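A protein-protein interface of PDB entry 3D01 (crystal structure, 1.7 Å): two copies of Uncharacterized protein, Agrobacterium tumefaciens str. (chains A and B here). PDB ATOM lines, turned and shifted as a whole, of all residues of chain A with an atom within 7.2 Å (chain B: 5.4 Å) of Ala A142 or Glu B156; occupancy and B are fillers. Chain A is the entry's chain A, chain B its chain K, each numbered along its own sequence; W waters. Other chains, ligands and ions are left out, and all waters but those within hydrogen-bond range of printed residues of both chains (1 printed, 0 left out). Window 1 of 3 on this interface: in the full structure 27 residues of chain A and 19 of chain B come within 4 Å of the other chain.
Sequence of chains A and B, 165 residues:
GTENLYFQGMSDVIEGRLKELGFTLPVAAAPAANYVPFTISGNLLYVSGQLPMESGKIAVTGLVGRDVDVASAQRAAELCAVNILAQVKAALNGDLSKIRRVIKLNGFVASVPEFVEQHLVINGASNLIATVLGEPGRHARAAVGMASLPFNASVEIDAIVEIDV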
ATOM      1  N   LYS A 104      13.338  -5.721  -5.995  1.00  0.00           N
ATOM      2  CA  LYS A 104      11.911  -5.645  -6.264  1.00  0.00           C
ATOM      3  C   LYS A 104      11.219  -4.646  -5.352  1.00  0.00           C
ATOM      4  O   LYS A 104      11.522  -4.546  -4.163  1.00  0.00           O
ATOM      5  CB  LYS A 104      11.285  -7.030  -6.129  1.00  0.00           C
ATOM      6  CG  LYS A 104       9.806  -7.053  -6.495  1.00  0.00           C
ATOM      7  CD  LYS A 104       9.398  -8.331  -7.120  1.00  0.00           C
ATOM      8  CE  LYS A 104       7.884  -8.379  -7.401  1.00  0.00           C
ATOM      9  NZ  LYS A 104       7.703  -7.272  -8.310  1.00  0.00           N
ATOM     10  N   LEU A 105      10.299  -3.895  -5.940  1.00  0.00           N
ATOM     11  CA  LEU A 105       9.332  -3.084  -5.203  1.00  0.00           C
ATOM     12  C   LEU A 105       7.949  -3.612  -5.522  1.00  0.00           C
ATOM     13  O   LEU A 105       7.649  -3.874  -6.682  1.00  0.00           O
ATOM     14  CB  LEU A 105       9.392  -1.594  -5.588  1.00  0.00           C
ATOM     15  CG  LEU A 105      10.676  -0.810  -5.315  1.00  0.00           C
ATOM     16  CD1 LEU A 105      10.409   0.636  -5.693  1.00  0.00           C
ATOM     17  CD2 LEU A 105      11.171  -0.933  -3.898  1.00  0.00           C
ATOM     18  N   ASN A 106       7.122  -3.765  -4.492  1.00  0.00           N
ATOM     19  CA  ASN A 106       5.706  -4.051  -4.700  1.00  0.00           C
ATOM     20  C   ASN A 106       4.928  -2.773  -4.340  1.00  0.00           C
ATOM     21  O   ASN A 106       4.926  -2.354  -3.189  1.00  0.00           O
ATOM     22  CB  ASN A 106       5.246  -5.266  -3.885  1.00  0.00           C
ATOM     23  CG  ASN A 106       5.957  -6.547  -4.302  1.00  0.00           C
ATOM     24  OD1 ASN A 106       6.748  -7.112  -3.536  1.00  0.00           O
ATOM     25  ND2 ASN A 106       5.684  -7.008  -5.511  1.00  0.00           N
ATOM     26  N   GLY A 107       4.285  -2.186  -5.343  1.00  0.00           N
ATOM     27  CA  GLY A 107       3.556  -0.929  -5.211  1.00  0.00           C
ATOM     28  C   GLY A 107       2.053  -1.158  -5.181  1.00  0.00           C
ATOM     29  O   GLY A 107       1.464  -1.604  -6.182  1.00  0.00           O
ATOM     30  N   PHE A 108       1.462  -0.837  -4.035  1.00  0.00           N
ATOM     31  CA  PHE A 108       0.069  -1.011  -3.754  1.00  0.00           C
ATOM     32  C   PHE A 108      -0.591   0.339  -3.715  1.00  0.00           C
ATOM     33  O   PHE A 108      -0.252   1.183  -2.848  1.00  0.00           O
ATOM     34  CB  PHE A 108      -0.107  -1.707  -2.401  1.00  0.00           C
ATOM     35  CG  PHE A 108       0.684  -2.991  -2.254  1.00  0.00           C
ATOM     36  CD1 PHE A 108       0.450  -4.070  -3.093  1.00  0.00           C
ATOM     37  CD2 PHE A 108       1.646  -3.110  -1.289  1.00  0.00           C
ATOM     38  CE1 PHE A 108       1.163  -5.244  -2.941  1.00  0.00           C
ATOM     39  CE2 PHE A 108       2.361  -4.292  -1.147  1.00  0.00           C
ATOM     40  CZ  PHE A 108       2.116  -5.334  -1.969  1.00  0.00           C
ATOM     41  N   GLN A 118      -1.991   2.883 -12.058  1.00  0.00           N
ATOM     42  CA  GLN A 118      -1.136   2.552 -10.926  1.00  0.00           C
ATOM     43  C   GLN A 118       0.342   2.500 -11.306  1.00  0.00           C
ATOM     44  O   GLN A 118       1.197   2.755 -10.443  1.00  0.00           O
ATOM     45  CB  GLN A 118      -1.534   1.242 -10.295  1.00  0.00           C
ATOM     46  CG  GLN A 118      -2.958   1.154  -9.704  1.00  0.00           C
ATOM     47  CD  GLN A 118      -4.026   0.881 -10.727  1.00  0.00           C
ATOM     48  OE1 GLN A 118      -3.739   0.754 -11.971  1.00  0.00           O
ATOM     49  NE2 GLN A 118      -5.271   0.822 -10.254  1.00  0.00           N
ATOM     50  N   ILE A 122       3.248   4.478  -9.151  1.00  0.00           N
ATOM     51  CA  ILE A 122       4.462   3.852  -8.619  1.00  0.00           C
ATOM     52  C   ILE A 122       5.735   4.428  -9.294  1.00  0.00           C
ATOM     53  O   ILE A 122       6.824   4.397  -8.690  1.00  0.00           O
ATOM     54  CB  ILE A 122       4.419   2.310  -8.709  1.00  0.00           C
ATOM     55  CG1 ILE A 122       3.193   1.794  -7.942  1.00  0.00           C
ATOM     56  CG2 ILE A 122       5.722   1.663  -8.160  1.00  0.00           C
ATOM     57  CD1 ILE A 122       3.068   2.291  -6.469  1.00  0.00           C
ATOM     58  N   HIS A 139      14.945  -1.679 -10.626  1.00  0.00           N
ATOM     59  CA  HIS A 139      14.363  -2.815  -9.922  1.00  0.00           C
ATOM     60  C   HIS A 139      13.245  -3.450 -10.729  1.00  0.00           C
ATOM     61  O   HIS A 139      12.667  -2.801 -11.607  1.00  0.00           O
ATOM     62  CB  HIS A 139      13.772  -2.300  -8.602  1.00  0.00           C
ATOM     63  CG  HIS A 139      12.998  -1.036  -8.779  1.00  0.00           C
ATOM     64  ND1 HIS A 139      13.608   0.204  -8.816  1.00  0.00           N
ATOM     65  CD2 HIS A 139      11.678  -0.815  -9.007  1.00  0.00           C
ATOM     66  CE1 HIS A 139      12.695   1.131  -9.045  1.00  0.00           C
ATOM     67  NE2 HIS A 139      11.517   0.541  -9.159  1.00  0.00           N
ATOM     68  N   ALA A 140      12.964  -4.718 -10.440  1.00  0.00           N
ATOM     69  CA  ALA A 140      11.714  -5.360 -10.853  1.00  0.00           C
ATOM     70  C   ALA A 140      10.583  -4.750 -10.016  1.00  0.00           C
ATOM     71  O   ALA A 140      10.829  -4.173  -8.980  1.00  0.00           O
ATOM     72  CB  ALA A 140      11.759  -6.836 -10.638  1.00  0.00           C
ATOM     73  N   ARG A 141       9.343  -4.917 -10.464  1.00  0.00           N
ATOM     74  CA  ARG A 141       8.221  -4.205  -9.869  1.00  0.00           C
ATOM     75  C   ARG A 141       6.871  -4.866 -10.136  1.00  0.00           C
ATOM     76  O   ARG A 141       6.673  -5.483 -11.182  1.00  0.00           O
ATOM     77  CB  ARG A 141       8.138  -2.814 -10.484  1.00  0.00           C
ATOM     78  CG  ARG A 141       7.526  -1.846  -9.596  1.00  0.00           C
ATOM     79  CD  ARG A 141       7.547  -0.447 -10.210  1.00  0.00           C
ATOM     80  NE  ARG A 141       6.569  -0.244 -11.291  1.00  0.00           N
ATOM     81  CZ  ARG A 141       6.349   0.949 -11.873  1.00  0.00           C
ATOM     82  NH1 ARG A 141       7.041   1.984 -11.499  1.00  0.00           N
ATOM     83  NH2 ARG A 141       5.445   1.108 -12.830  1.00  0.00           N
ATOM     84  N   ALA A 142       5.942  -4.716  -9.199  1.00  0.00           N
ATOM     85  CA  ALA A 142       4.514  -4.912  -9.482  1.00  0.00           C
ATOM     86  C   ALA A 142       3.794  -3.629  -9.038  1.00  0.00           C
ATOM     87  O   ALA A 142       4.221  -2.945  -8.102  1.00  0.00           O
ATOM     88  CB  ALA A 142       3.954  -6.140  -8.737  1.00  0.00           C
ATOM     89  N   ALA A 143       2.720  -3.277  -9.732  1.00  0.00           N
ATOM     90  CA  ALA A 143       1.926  -2.098  -9.396  1.00  0.00           C
ATOM     91  C   ALA A 143       0.468  -2.547  -9.563  1.00  0.00           C
ATOM     92  O   ALA A 143       0.061  -3.036 -10.654  1.00  0.00           O
ATOM     93  CB  ALA A 143       2.263  -0.926 -10.319  1.00  0.00           C
ATOM     94  N   VAL A 144      -0.296  -2.403  -8.482  1.00  0.00           N
ATOM     95  CA  VAL A 144      -1.637  -2.995  -8.398  1.00  0.00           C
ATOM     96  C   VAL A 144      -2.570  -2.069  -7.633  1.00  0.00           C
ATOM     97  O   VAL A 144      -2.123  -1.228  -6.828  1.00  0.00           O
ATOM     98  CB  VAL A 144      -1.559  -4.378  -7.759  1.00  0.00           C
ATOM     99  CG1 VAL A 144      -0.828  -5.327  -8.697  1.00  0.00           C
ATOM    100  CG2 VAL A 144      -0.906  -4.314  -6.341  1.00  0.00           C
ATOM    101  N   GLY A 145      -3.852  -2.208  -7.925  1.00  0.00           N
ATOM    102  CA  GLY A 145      -4.889  -1.404  -7.311  1.00  0.00           C
ATOM    103  C   GLY A 145      -5.611  -2.113  -6.183  1.00  0.00           C
ATOM    104  O   GLY A 145      -6.236  -3.178  -6.391  1.00  0.00           O
ATOM    105  N   ILE A 157       4.258   0.607  -0.198  1.00  0.00           N
ATOM    106  CA  ILE A 157       5.278  -0.048  -1.033  1.00  0.00           C
ATOM    107  C   ILE A 157       6.206  -0.850  -0.157  1.00  0.00           C
ATOM    108  O   ILE A 157       6.687  -0.336   0.840  1.00  0.00           O
ATOM    109  CB  ILE A 157       6.129   1.010  -1.851  1.00  0.00           C
ATOM    110  CG1 ILE A 157       5.214   1.945  -2.687  1.00  0.00           C
ATOM    111  CG2 ILE A 157       7.145   0.310  -2.757  1.00  0.00           C
ATOM    112  CD1 ILE A 157       5.957   2.929  -3.628  1.00  0.00           C
ATOM    113  N   SER B  48       9.085  -8.883 -13.043  1.00  0.00           N
ATOM    114  CA  SER B  48       8.050  -7.840 -12.811  1.00  0.00           C
ATOM    115  C   SER B  48       6.639  -8.325 -13.192  1.00  0.00           C
ATOM    116  O   SER B  48       6.478  -9.245 -14.023  1.00  0.00           O
ATOM    117  CB  SER B  48       8.385  -6.600 -13.641  1.00  0.00           C
ATOM    118  OG  SER B  48       9.510  -5.971 -13.107  1.00  0.00           O
ATOM    119  N   GLY B  49       5.611  -7.732 -12.579  1.00  0.00           N
ATOM    120  CA  GLY B  49       4.235  -8.031 -12.982  1.00  0.00           C
ATOM    121  C   GLY B  49       4.049  -7.903 -14.482  1.00  0.00           C
ATOM    122  O   GLY B  49       4.349  -6.855 -15.070  1.00  0.00           O
ATOM    123  N   GLN B  50       3.553  -8.979 -15.084  1.00  0.00           N
ATOM    124  CA  GLN B  50       3.222  -9.042 -16.499  1.00  0.00           C
ATOM    125  C   GLN B  50       1.711  -8.941 -16.665  1.00  0.00           C
ATOM    126  O   GLN B  50       0.939  -9.517 -15.889  1.00  0.00           O
ATOM    127  CB  GLN B  50       3.746 -10.349 -17.143  1.00  0.00           C
ATOM    128  CG  GLN B  50       5.284 -10.507 -17.009  1.00  0.00           C
ATOM    129  CD  GLN B  50       6.050  -9.414 -17.733  1.00  0.00           C
ATOM    130  OE1 GLN B  50       5.846  -9.196 -18.939  1.00  0.00           O
ATOM    131  NE2 GLN B  50       6.937  -8.724 -17.020  1.00  0.00           N
ATOM    132  N   LEU B  51       1.333  -8.216 -17.702  1.00  0.00           N
ATOM    133  CA  LEU B  51      -0.057  -7.990 -18.105  1.00  0.00           C
ATOM    134  C   LEU B  51      -0.382  -8.968 -19.256  1.00  0.00           C
ATOM    135  O   LEU B  51       0.523  -9.623 -19.797  1.00  0.00           O
ATOM    136  CB  LEU B  51      -0.206  -6.520 -18.541  1.00  0.00           C
ATOM    137  CG  LEU B  51       0.210  -5.494 -17.467  1.00  0.00           C
ATOM    138  CD1 LEU B  51       0.117  -4.036 -17.899  1.00  0.00           C
ATOM    139  CD2 LEU B  51      -0.578  -5.697 -16.163  1.00  0.00           C
ATOM    140  N   CYS B  80      -0.507 -13.506 -19.414  1.00  0.00           N
ATOM    141  CA  CYS B  80       0.448 -13.087 -18.373  1.00  0.00           C
ATOM    142  C   CYS B  80       1.594 -14.095 -18.237  1.00  0.00           C
ATOM    143  O   CYS B  80       2.746 -13.687 -18.168  1.00  0.00           O
ATOM    144  CB  CYS B  80      -0.211 -12.906 -17.003  1.00  0.00           C
ATOM    145  SG  CYS B  80      -1.461 -11.594 -16.942  1.00  0.00           S
ATOM    146  N   ASN B 106       2.658 -14.647  -8.060  1.00  0.00           N
ATOM    147  CA  ASN B 106       1.621 -13.819  -7.419  1.00  0.00           C
ATOM    148  C   ASN B 106       0.625 -13.400  -8.473  1.00  0.00           C
ATOM    149  O   ASN B 106       0.966 -12.657  -9.373  1.00  0.00           O
ATOM    150  CB  ASN B 106       2.233 -12.611  -6.721  1.00  0.00           C
ATOM    151  CG  ASN B 106       3.217 -13.012  -5.611  1.00  0.00           C
ATOM    152  OD1 ASN B 106       4.419 -12.730  -5.698  1.00  0.00           O
ATOM    153  ND2 ASN B 106       2.717 -13.674  -4.593  1.00  0.00           N
ATOM    154  N   GLY B 107      -0.599 -13.895  -8.350  1.00  0.00           N
ATOM    155  CA  GLY B 107      -1.633 -13.647  -9.316  1.00  0.00           C
ATOM    156  C   GLY B 107      -2.625 -12.630  -8.802  1.00  0.00           C
ATOM    157  O   GLY B 107      -3.335 -12.887  -7.847  1.00  0.00           O
ATOM    158  N   PHE B 108      -2.639 -11.480  -9.458  1.00  0.00           N
ATOM    159  CA  PHE B 108      -3.495 -10.369  -9.115  1.00  0.00           C
ATOM    160  C   PHE B 108      -4.642 -10.308 -10.133  1.00  0.00           C
ATOM    161  O   PHE B 108      -4.385 -10.158 -11.330  1.00  0.00           O
ATOM    162  CB  PHE B 108      -2.653  -9.103  -9.170  1.00  0.00           C
ATOM    163  CG  PHE B 108      -1.408  -9.174  -8.332  1.00  0.00           C
ATOM    164  CD1 PHE B 108      -1.516  -9.254  -6.982  1.00  0.00           C
ATOM    165  CD2 PHE B 108      -0.150  -9.071  -8.882  1.00  0.00           C
ATOM    166  CE1 PHE B 108      -0.399  -9.281  -6.186  1.00  0.00           C
ATOM    167  CE2 PHE B 108       0.978  -9.094  -8.077  1.00  0.00           C
ATOM    168  CZ  PHE B 108       0.831  -9.201  -6.730  1.00  0.00           C
ATOM    169  N   VAL B 109      -5.889 -10.429  -9.652  1.00  0.00           N
ATOM    170  CA  VAL B 109      -7.068 -10.512 -10.546  1.00  0.00           C
ATOM    171  C   VAL B 109      -8.008  -9.311 -10.267  1.00  0.00           C
ATOM    172  O   VAL B 109      -8.552  -9.204  -9.179  1.00  0.00           O
ATOM    173  CB  VAL B 109      -7.869 -11.799 -10.299  1.00  0.00           C
ATOM    174  CG1 VAL B 109      -9.055 -11.845 -11.276  1.00  0.00           C
ATOM    175  CG2 VAL B 109      -6.953 -13.051 -10.391  1.00  0.00           C
ATOM    176  N   LEU B 149      -6.277  -2.667 -12.149  1.00  0.00           N
ATOM    177  CA  LEU B 149      -4.876  -2.915 -12.539  1.00  0.00           C
ATOM    178  C   LEU B 149      -4.468  -1.929 -13.622  1.00  0.00           C
ATOM    179  O   LEU B 149      -5.346  -1.350 -14.291  1.00  0.00           O
ATOM    180  CB  LEU B 149      -4.700  -4.355 -13.040  1.00  0.00           C
ATOM    181  CG  LEU B 149      -4.891  -5.478 -12.025  1.00  0.00           C
ATOM    182  CD1 LEU B 149      -4.907  -6.849 -12.734  1.00  0.00           C
ATOM    183  CD2 LEU B 149      -3.756  -5.410 -10.953  1.00  0.00           C
ATOM    184  N   PRO B 150      -3.144  -1.718 -13.809  1.00  0.00           N
ATOM    185  CA  PRO B 150      -2.659  -0.876 -14.902  1.00  0.00           C
ATOM    186  C   PRO B 150      -3.228  -1.206 -16.266  1.00  0.00           C
ATOM    187  O   PRO B 150      -3.331  -2.410 -16.648  1.00  0.00           O
ATOM    188  CB  PRO B 150      -1.154  -1.146 -14.907  1.00  0.00           C
ATOM    189  CG  PRO B 150      -0.849  -1.395 -13.454  1.00  0.00           C
ATOM    190  CD  PRO B 150      -2.020  -2.181 -12.969  1.00  0.00           C
ATOM    191  N   ALA B 153      -5.936  -3.905 -17.207  1.00  0.00           N
ATOM    192  CA  ALA B 153      -5.709  -5.345 -17.335  1.00  0.00           C
ATOM    193  C   ALA B 153      -6.630  -6.110 -16.360  1.00  0.00           C
ATOM    194  O   ALA B 153      -6.855  -5.669 -15.215  1.00  0.00           O
ATOM    195  CB  ALA B 153      -4.273  -5.686 -17.062  1.00  0.00           C
ATOM    196  N   SER B 154      -7.144  -7.262 -16.802  1.00  0.00           N
ATOM    197  CA  SER B 154      -7.963  -8.099 -15.920  1.00  0.00           C
ATOM    198  C   SER B 154      -7.100  -8.895 -14.928  1.00  0.00           C
ATOM    199  O   SER B 154      -7.572  -9.272 -13.875  1.00  0.00           O
ATOM    200  CB  SER B 154      -8.846  -9.045 -16.725  1.00  0.00           C
ATOM    201  OG  SER B 154      -9.743  -8.303 -17.519  1.00  0.00           O
ATOM    202  N   VAL B 155      -5.851  -9.171 -15.311  1.00  0.00           N
ATOM    203  CA  VAL B 155      -4.912  -9.995 -14.521  1.00  0.00           C
ATOM    204  C   VAL B 155      -3.489  -9.435 -14.708  1.00  0.00           C
ATOM    205  O   VAL B 155      -3.089  -9.040 -15.839  1.00  0.00           O
ATOM    206  CB  VAL B 155      -4.924 -11.511 -14.972  1.00  0.00           C
ATOM    207  CG1 VAL B 155      -4.006 -12.402 -14.071  1.00  0.00           C
ATOM    208  CG2 VAL B 155      -6.371 -12.067 -15.108  1.00  0.00           C
ATOM    209  N   GLU B 156      -2.727  -9.443 -13.621  1.00  0.00           N
ATOM    210  CA  GLU B 156      -1.287  -9.151 -13.617  1.00  0.00           C
ATOM    211  C   GLU B 156      -0.627 -10.235 -12.780  1.00  0.00           C
ATOM    212  O   GLU B 156      -1.134 -10.583 -11.717  1.00  0.00           O
ATOM    213  CB  GLU B 156      -1.008  -7.791 -12.996  1.00  0.00           C
ATOM    214  CG  GLU B 156       0.451  -7.418 -12.883  1.00  0.00           C
ATOM    215  CD  GLU B 156       0.666  -6.076 -12.200  1.00  0.00           C
ATOM    216  OE1 GLU B 156      -0.224  -5.212 -12.261  1.00  0.00           O
ATOM    217  OE2 GLU B 156       1.751  -5.874 -11.619  1.00  0.00           O
ATOM    218  N   ILE B 157       0.488 -10.770 -13.249  1.00  0.00           N
ATOM    219  CA  ILE B 157       1.154 -11.856 -12.528  1.00  0.00           C
ATOM    220  C   ILE B 157       2.650 -11.613 -12.487  1.00  0.00           C
ATOM    221  O   ILE B 157       3.254 -11.316 -13.533  1.00  0.00           O
ATOM    222  CB  ILE B 157       0.903 -13.252 -13.178  1.00  0.00           C
ATOM    223  CG1 ILE B 157      -0.595 -13.552 -13.403  1.00  0.00           C
ATOM    224  CG2 ILE B 157       1.528 -14.366 -12.279  1.00  0.00           C
ATOM    225  CD1 ILE B 157      -0.834 -14.939 -14.055  1.00  0.00           C
ATOM    226  N   ASP B 158       3.244 -11.715 -11.293  1.00  0.00           N
ATOM    227  CA  ASP B 158       4.689 -11.642 -11.149  1.00  0.00           C
ATOM    228  C   ASP B 158       5.228 -13.015 -10.793  1.00  0.00           C
ATOM    229  O   ASP B 158       4.453 -13.955 -10.528  1.00  0.00           O
ATOM    230  CB  ASP B 158       5.126 -10.519 -10.196  1.00  0.00           C
ATOM    231  CG  ASP B 158       4.870 -10.792  -8.723  1.00  0.00           C
ATOM    232  OD1 ASP B 158       4.654 -11.944  -8.311  1.00  0.00           O
ATOM    233  OD2 ASP B 158       4.885  -9.792  -7.954  1.00  0.00           O
HETATM  234  O   HOH W   1       4.374  -9.186  -5.513  1.00  0.00           O
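NZ of Lys A104 is in salt-bridge range of OD2 of Asp B158, 3.8 Å away. OE1 of Gln A118 sits close to N of Pro B150. The backbone carbonyl oxygen (O) of Arg A141 lies within hydrogen-bond range of the backbone NH (N) of Gly B49, at 2.9 Å. OG of Ser B48 sits at hydrogen-bond distance from N of Arg A141 (2.9 Å). N of Ala A143 is in hydrogen-bond range of OE2 of Glu B156, 3.4 Å away.
The backbone NH of Leu A105 sits at hydrogen-bond distance from the backbone carbonyl oxygen of Ala A140, 3.1 Å away. The backbone NH of Gly A107 is in hydrogen-bond range of the backbone carbonyl oxygen of Ala A142 (2.9 Å). OD1 of Asp B158 sits close to OD1 of Asn B106. The backbone NH (N) of Val A144 is in hydrogen-bond range of the backbone carbonyl oxygen (O) of Gly A107 (3.0 Å). The backbone carbonyl oxygen (O) of Glu B156 lies within hydrogen-bond range of the backbone NH (N) of Phe B108. The side-chain amino group of Lys A104 lies close to the side-chain amide nitrogen of Asn A106, 3.5 Å away.
Asn A106 touches Asp B158 (ND2 to OD2, 3.8 Å). Gln A118 touches Leu B149. Ala A140 touches Ser B48. Ala A142 touches Glu B156. OD2 of Asp B158 touches CB of Ala A142, at 3.8 Å. Ala A143 touches Pro B150. Phe B108 touches Val A144. Leu B149 touches Val A144 (CD2 to CG1, 3.7 Å). CG1 of Val A144 touches OE1 of Glu B156, at 3.6 Å.
Ala A142 touches just these residues of chain B: Glu B156 and Asp B158. Glu B156 touches just these residues of chain A: Ala A142, Ala A143 and Val A144. Of the printed residues of chain A, Pro B150 touches Gln A118 (3.1 Å) and Ala A143 (3.2 Å). Of the printed residues of chain B, Asn A106 touches Asp B158 (3.8 Å). Of the printed residues of chain B, Lys A104 touches Asp B158. Of the printed residues of chain B, Val A144 touches Phe B108, Leu B149 and Glu B156. Printed residues of chain A within 4 Å of Asp B158: Lys A104 (3.4 Å), Asn A106 (3.8 Å) and Ala A142 (3.8 Å). Gly A107 touches none of the printed residues of chain B. Ile B157 touches none of the printed residues of chain A. The nearest residue of chain A that does not touch Glu B156 is Arg A141 (5.0 Å).
Of the 17 printed residues of chain B, 7 touch a printed residue of chain A. Printed residues of chain B that touch a printed residue of chain A: Ser B48, Gly B49, Phe B108, Leu B149, Pro B150, Glu B156 and Asp B158. Among the printed residues, 14 pairs touch across the chains. Among the printed residues, Asp or Glu carboxylates within 4 Å of a Lys or Arg side-chain nitrogen of the other chain: Lys A104 with Asp B158 (3.8 Å).
Positions printed for both chains: 106, 107, 108 and 157.
Water W1 bridges the side-chain amide nitrogen (ND2) of Asn A106 (2.5 Å) and the side-chain carboxylate (OD2) of Asp B158 (2.6 Å).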
